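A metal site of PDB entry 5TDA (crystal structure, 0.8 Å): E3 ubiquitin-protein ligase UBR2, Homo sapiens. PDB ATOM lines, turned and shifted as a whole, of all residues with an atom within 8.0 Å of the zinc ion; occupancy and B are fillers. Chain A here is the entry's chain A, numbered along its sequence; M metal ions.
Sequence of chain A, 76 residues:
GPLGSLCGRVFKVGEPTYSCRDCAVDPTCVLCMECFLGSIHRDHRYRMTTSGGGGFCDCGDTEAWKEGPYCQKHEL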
ATOM      1  N   SER A  19     -16.415   8.581   5.654  1.00  0.00           N
ATOM      2  CA  SER A  19     -17.150   7.990   6.759  1.00  0.00           C
ATOM      3  C   SER A  19     -16.292   6.904   7.387  1.00  0.00           C
ATOM      4  O   SER A  19     -15.585   6.191   6.691  1.00  0.00           O
ATOM      5  CB  SER A  19     -18.500   7.403   6.312  1.00  0.00           C
ATOM      6  OG  SER A  19     -19.206   6.945   7.451  1.00  0.00           O
ATOM      7  N   CYS A  20     -16.359   6.775   8.703  1.00  0.00           N
ATOM      8  CA  CYS A  20     -15.700   5.677   9.401  1.00  0.00           C
ATOM      9  C   CYS A  20     -16.644   4.489   9.447  1.00  0.00           C
ATOM     10  O   CYS A  20     -17.706   4.565  10.088  1.00  0.00           O
ATOM     11  CB  CYS A  20     -15.292   6.054  10.831  1.00  0.00           C
ATOM     12  SG  CYS A  20     -14.366   4.640  11.509  1.00  0.00           S
ATOM     13  N   ARG A  21     -16.282   3.405   8.751  1.00  0.00           N
ATOM     14  CA  ARG A  21     -17.138   2.217   8.748  1.00  0.00           C
ATOM     15  C   ARG A  21     -17.219   1.580  10.133  1.00  0.00           C
ATOM     16  O   ARG A  21     -18.235   0.947  10.461  1.00  0.00           O
ATOM     17  CB  ARG A  21     -16.634   1.236   7.696  1.00  0.00           C
ATOM     18  CG  ARG A  21     -16.710   1.760   6.257  1.00  0.00           C
ATOM     19  CD  ARG A  21     -15.808   0.993   5.283  1.00  0.00           C
ATOM     20  NE  ARG A  21     -16.231  -0.398   5.131  1.00  0.00           N
ATOM     21  CZ  ARG A  21     -15.482  -1.384   4.622  1.00  0.00           C
ATOM     22  NH1 ARG A  21     -14.245  -1.141   4.217  1.00  0.00           N
ATOM     23  NH2 ARG A  21     -15.973  -2.615   4.531  1.00  0.00           N
ATOM     24  N   ASP A  22     -16.184   1.739  10.957  1.00  0.00           N
ATOM     25  CA  ASP A  22     -16.157   1.143  12.285  1.00  0.00           C
ATOM     26  C   ASP A  22     -17.039   1.903  13.282  1.00  0.00           C
ATOM     27  O   ASP A  22     -17.697   1.296  14.136  1.00  0.00           O
ATOM     28  CB  ASP A  22     -14.716   1.055  12.801  1.00  0.00           C
ATOM     29  CG  ASP A  22     -13.822   0.160  11.942  1.00  0.00           C
ATOM     30  OD1 ASP A  22     -12.647   0.515  11.717  1.00  0.00           O
ATOM     31  OD2 ASP A  22     -14.283  -0.912  11.534  1.00  0.00           O
ATOM     32  N   CYS A  23     -17.040   3.249  13.211  1.00  0.00           N
ATOM     33  CA  CYS A  23     -17.617   4.076  14.253  1.00  0.00           C
ATOM     34  C   CYS A  23     -18.918   4.786  13.879  1.00  0.00           C
ATOM     35  O   CYS A  23     -19.625   5.255  14.790  1.00  0.00           O
ATOM     36  CB  CYS A  23     -16.595   5.140  14.723  1.00  0.00           C
ATOM     37  SG  CYS A  23     -15.033   4.446  15.348  1.00  0.00           S
ATOM     38  N   ALA A  24     -19.231   4.922  12.593  1.00  0.00           N
ATOM     39  CA  ALA A  24     -20.440   5.636  12.204  1.00  0.00           C
ATOM     40  C   ALA A  24     -21.672   4.960  12.791  1.00  0.00           C
ATOM     41  O   ALA A  24     -21.815   3.739  12.700  1.00  0.00           O
ATOM     42  CB  ALA A  24     -20.595   5.682  10.681  1.00  0.00           C
ATOM     43  N   LEU A  31     -17.629  12.920   7.564  1.00  0.00           N
ATOM     44  CA  LEU A  31     -16.703  13.964   7.990  1.00  0.00           C
ATOM     45  C   LEU A  31     -16.046  14.604   6.753  1.00  0.00           C
ATOM     46  O   LEU A  31     -15.771  13.935   5.760  1.00  0.00           O
ATOM     47  CB  LEU A  31     -15.576  13.379   8.864  1.00  0.00           C
ATOM     48  CG  LEU A  31     -16.037  12.741  10.175  1.00  0.00           C
ATOM     49  CD1 LEU A  31     -14.910  11.983  10.856  1.00  0.00           C
ATOM     50  CD2 LEU A  31     -16.628  13.777  11.123  1.00  0.00           C
ATOM     51  N   PHE A  36     -11.792  14.414   9.348  1.00  0.00           N
ATOM     52  CA  PHE A  36     -11.400  13.004   9.269  1.00  0.00           C
ATOM     53  C   PHE A  36      -9.922  12.823   9.621  1.00  0.00           C
ATOM     54  O   PHE A  36      -9.570  11.994  10.479  1.00  0.00           O
ATOM     55  CB  PHE A  36     -11.691  12.452   7.865  1.00  0.00           C
ATOM     56  CG  PHE A  36     -11.249  11.023   7.703  1.00  0.00           C
ATOM     57  CD1 PHE A  36     -11.953  10.001   8.319  1.00  0.00           C
ATOM     58  CD2 PHE A  36     -10.106  10.707   6.985  1.00  0.00           C
ATOM     59  CE1 PHE A  36     -11.544   8.680   8.200  1.00  0.00           C
ATOM     60  CE2 PHE A  36      -9.678   9.386   6.858  1.00  0.00           C
ATOM     61  CZ  PHE A  36     -10.405   8.366   7.473  1.00  0.00           C
ATOM     62  N   SER A  39      -8.916  13.212  13.242  1.00  0.00           N
ATOM     63  CA  SER A  39      -9.661  12.365  14.159  1.00  0.00           C
ATOM     64  C   SER A  39      -8.993  11.000  14.287  1.00  0.00           C
ATOM     65  O   SER A  39      -8.106  10.630  13.484  1.00  0.00           O
ATOM     66  CB  SER A  39     -11.105  12.153  13.651  1.00  0.00           C
ATOM     67  OG  SER A  39     -11.157  11.206  12.598  1.00  0.00           O
ATOM     68  N   ILE A  40      -9.466  10.223  15.252  1.00  0.00           N
ATOM     69  CA  ILE A  40      -9.018   8.848  15.450  1.00  0.00           C
ATOM     70  C   ILE A  40      -9.298   7.990  14.216  1.00  0.00           C
ATOM     71  O   ILE A  40      -8.649   6.954  13.982  1.00  0.00           O
ATOM     72  CB  ILE A  40      -9.683   8.270  16.741  1.00  0.00           C
ATOM     73  CG1 ILE A  40      -8.958   7.010  17.199  1.00  0.00           C
ATOM     74  CG2 ILE A  40     -11.165   7.981  16.554  1.00  0.00           C
ATOM     75  CD1 ILE A  40      -7.590   7.268  17.728  1.00  0.00           C
ATOM     76  N   HIS A  41     -10.315   8.376  13.431  1.00  0.00           N
ATOM     77  CA  HIS A  41     -10.808   7.528  12.358  1.00  0.00           C
ATOM     78  C   HIS A  41      -9.833   7.403  11.192  1.00  0.00           C
ATOM     79  O   HIS A  41     -10.005   6.504  10.360  1.00  0.00           O
ATOM     80  CB  HIS A  41     -12.188   8.011  11.889  1.00  0.00           C
ATOM     81  CG  HIS A  41     -13.130   8.241  13.025  1.00  0.00           C
ATOM     82  ND1 HIS A  41     -13.625   7.226  13.823  1.00  0.00           N
ATOM     83  CD2 HIS A  41     -13.581   9.409  13.535  1.00  0.00           C
ATOM     84  CE1 HIS A  41     -14.355   7.781  14.778  1.00  0.00           C
ATOM     85  NE2 HIS A  41     -14.357   9.092  14.631  1.00  0.00           N
ATOM     86  N   ARG A  42      -8.807   8.244  11.129  1.00  0.00           N
ATOM     87  CA  ARG A  42      -7.804   8.091  10.077  1.00  0.00           C
ATOM     88  C   ARG A  42      -7.091   6.741  10.158  1.00  0.00           C
ATOM     89  O   ARG A  42      -6.494   6.302   9.168  1.00  0.00           O
ATOM     90  CB  ARG A  42      -6.804   9.249  10.089  1.00  0.00           C
ATOM     91  CG  ARG A  42      -5.817   9.218  11.240  1.00  0.00           C
ATOM     92  CD  ARG A  42      -4.979  10.478  11.248  1.00  0.00           C
ATOM     93  NE  ARG A  42      -3.923  10.481  12.256  1.00  0.00           N
ATOM     94  CZ  ARG A  42      -3.368  11.578  12.777  1.00  0.00           C
ATOM     95  NH1 ARG A  42      -3.752  12.788  12.406  1.00  0.00           N
ATOM     96  NH2 ARG A  42      -2.414  11.451  13.680  1.00  0.00           N
ATOM     97  N   ASP A  43      -7.138   6.077  11.319  1.00  0.00           N
ATOM     98  CA  ASP A  43      -6.538   4.762  11.491  1.00  0.00           C
ATOM     99  C   ASP A  43      -7.560   3.634  11.451  1.00  0.00           C
ATOM    100  O   ASP A  43      -7.211   2.492  11.765  1.00  0.00           O
ATOM    101  CB  ASP A  43      -5.745   4.719  12.799  1.00  0.00           C
ATOM    102  CG  ASP A  43      -4.549   5.625  12.772  1.00  0.00           C
ATOM    103  OD1 ASP A  43      -3.890   5.719  11.721  1.00  0.00           O
ATOM    104  OD2 ASP A  43      -4.274   6.272  13.805  1.00  0.00           O
ATOM    105  N   HIS A  44      -8.805   3.935  11.077  1.00  0.00           N
ATOM    106  CA  HIS A  44      -9.884   2.961  11.026  1.00  0.00           C
ATOM    107  C   HIS A  44     -10.247   2.645   9.571  1.00  0.00           C
ATOM    108  O   HIS A  44      -9.673   3.199   8.626  1.00  0.00           O
ATOM    109  CB  HIS A  44     -11.105   3.526  11.778  1.00  0.00           C
ATOM    110  CG  HIS A  44     -10.880   3.720  13.247  1.00  0.00           C
ATOM    111  ND1 HIS A  44     -11.804   4.363  14.051  1.00  0.00           N
ATOM    112  CD2 HIS A  44      -9.863   3.339  14.055  1.00  0.00           C
ATOM    113  CE1 HIS A  44     -11.354   4.364  15.294  1.00  0.00           C
ATOM    114  NE2 HIS A  44     -10.179   3.755  15.322  1.00  0.00           N
ATOM    115  N   ARG A  45     -11.220   1.750   9.383  1.00  0.00           N
ATOM    116  CA  ARG A  45     -11.730   1.448   8.040  1.00  0.00           C
ATOM    117  C   ARG A  45     -12.659   2.578   7.622  1.00  0.00           C
ATOM    118  O   ARG A  45     -13.538   2.964   8.393  1.00  0.00           O
ATOM    119  CB  ARG A  45     -12.513   0.133   8.061  1.00  0.00           C
ATOM    120  CG  ARG A  45     -11.672  -1.073   8.406  1.00  0.00           C
ATOM    121  CD  ARG A  45     -12.499  -2.329   8.372  1.00  0.00           C
ATOM    122  NE  ARG A  45     -13.660  -2.208   9.235  1.00  0.00           N
ATOM    123  CZ  ARG A  45     -14.895  -2.564   8.891  1.00  0.00           C
ATOM    124  NH1 ARG A  45     -15.156  -3.085   7.707  1.00  0.00           N
ATOM    125  NH2 ARG A  45     -15.873  -2.385   9.771  1.00  0.00           N
ATOM    126  N   TYR A  46     -12.475   3.108   6.433  1.00  0.00           N
ATOM    127  CA  TYR A  46     -13.246   4.264   6.000  1.00  0.00           C
ATOM    128  C   TYR A  46     -13.766   4.073   4.579  1.00  0.00           C
ATOM    129  O   TYR A  46     -13.324   3.207   3.830  1.00  0.00           O
ATOM    130  CB  TYR A  46     -12.414   5.547   6.095  1.00  0.00           C
ATOM    131  CG  TYR A  46     -11.198   5.561   5.200  1.00  0.00           C
ATOM    132  CD1 TYR A  46      -9.959   5.146   5.669  1.00  0.00           C
ATOM    133  CD2 TYR A  46     -11.284   5.979   3.871  1.00  0.00           C
ATOM    134  CE1 TYR A  46      -8.848   5.152   4.861  1.00  0.00           C
ATOM    135  CE2 TYR A  46     -10.177   5.978   3.052  1.00  0.00           C
ATOM    136  CZ  TYR A  46      -8.961   5.571   3.544  1.00  0.00           C
ATOM    137  OH  TYR A  46      -7.847   5.565   2.743  1.00  0.00           O
ATOM    138  N   TRP A  65     -21.418   9.210  16.135  1.00  0.00           N
ATOM    139  CA  TRP A  65     -20.170   8.448  16.214  1.00  0.00           C
ATOM    140  C   TRP A  65     -20.160   7.643  17.515  1.00  0.00           C
ATOM    141  O   TRP A  65     -20.413   8.197  18.591  1.00  0.00           O
ATOM    142  CB  TRP A  65     -18.932   9.402  16.181  1.00  0.00           C
ATOM    143  CG  TRP A  65     -18.989  10.296  14.969  1.00  0.00           C
ATOM    144  CD1 TRP A  65     -19.341  11.622  14.942  1.00  0.00           C
ATOM    145  CD2 TRP A  65     -18.788   9.902  13.612  1.00  0.00           C
ATOM    146  NE1 TRP A  65     -19.360  12.077  13.640  1.00  0.00           N
ATOM    147  CE2 TRP A  65     -19.026  11.038  12.801  1.00  0.00           C
ATOM    148  CE3 TRP A  65     -18.442   8.690  12.989  1.00  0.00           C
ATOM    149  CZ2 TRP A  65     -18.946  10.999  11.400  1.00  0.00           C
ATOM    150  CZ3 TRP A  65     -18.357   8.648  11.598  1.00  0.00           C
ATOM    151  CH2 TRP A  65     -18.610   9.787  10.827  1.00  0.00           C
ATOM    152  N   LYS A  66     -19.819   6.357  17.412  1.00  0.00           N
ATOM    153  CA  LYS A  66     -19.776   5.483  18.591  1.00  0.00           C
ATOM    154  C   LYS A  66     -18.483   5.640  19.382  1.00  0.00           C
ATOM    155  O   LYS A  66     -18.404   5.218  20.545  1.00  0.00           O
ATOM    156  CB  LYS A  66     -19.969   4.028  18.143  1.00  0.00           C
ATOM    157  CG  LYS A  66     -21.343   3.786  17.497  1.00  0.00           C
ATOM    158  CD  LYS A  66     -21.557   2.343  17.051  1.00  0.00           C
ATOM    159  CE  LYS A  66     -20.904   2.044  15.728  1.00  0.00           C
ATOM    160  NZ  LYS A  66     -21.087   0.617  15.328  1.00  0.00           N
ATOM    161  N   GLU A  67     -17.464   6.225  18.760  1.00  0.00           N
ATOM    162  CA  GLU A  67     -16.175   6.586  19.328  1.00  0.00           C
ATOM    163  C   GLU A  67     -15.710   7.791  18.528  1.00  0.00           C
ATOM    164  O   GLU A  67     -16.071   7.938  17.355  1.00  0.00           O
ATOM    165  CB  GLU A  67     -15.160   5.430  19.165  1.00  0.00           C
ATOM    166  CG  GLU A  67     -13.819   5.658  19.888  1.00  0.00           C
ATOM    167  CD  GLU A  67     -12.752   4.583  19.612  1.00  0.00           C
ATOM    168  OE1 GLU A  67     -12.672   4.039  18.489  1.00  0.00           O
ATOM    169  OE2 GLU A  67     -11.963   4.304  20.545  1.00  0.00           O
ATOM    170  N   GLY A  68     -14.911   8.673  19.145  1.00  0.00           N
ATOM    171  CA  GLY A  68     -14.313   9.777  18.405  1.00  0.00           C
ATOM    172  C   GLY A  68     -15.299  10.722  17.738  1.00  0.00           C
ATOM    173  O   GLY A  68     -15.257  10.937  16.512  1.00  0.00           O
HETATM  174 ZN    ZN M   1     -13.654   5.168  13.635  1.00  0.00          ZN
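Four residues have an atom within 4 Å of the zinc ion: Cys 20, Cys 23, His 41 and His 44.
A ring nitrogen (NE2) of His 41 lies close to the backbone carbonyl oxygen (O) of Glu 67.
The side-chain hydroxyl (OG) of Ser 39 lies close to the backbone NH (N) of His 41, at 3.1 Å.
SG of Cys 20 lies close to N of Asp 22 (3.5 Å).
The backbone carbonyl oxygen (O) of Cys 23 sits at hydrogen-bond distance from the backbone NH (N) of Lys 66.
A ring nitrogen (NE2) of His 41 lies within hydrogen-bond range of the backbone carbonyl oxygen (O) of Gly 68, 2.8 Å away.
The side-chain sulfur (SG) of Cys 20 sits close to the backbone carbonyl oxygen (O) of Arg 45.
A ring nitrogen (ND1) of His 44 is bound to the zinc ion, 2.1 Å away.
ND1 of His 41 is bound to the zinc ion (2.1 Å).
The zinc ion is bound by SG of Cys 20, at 2.3 Å.
The side-chain sulfur (SG) of Cys 23 binds the zinc ion, 2.3 Å away.
The zinc ion has four donor atoms within binding distance.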
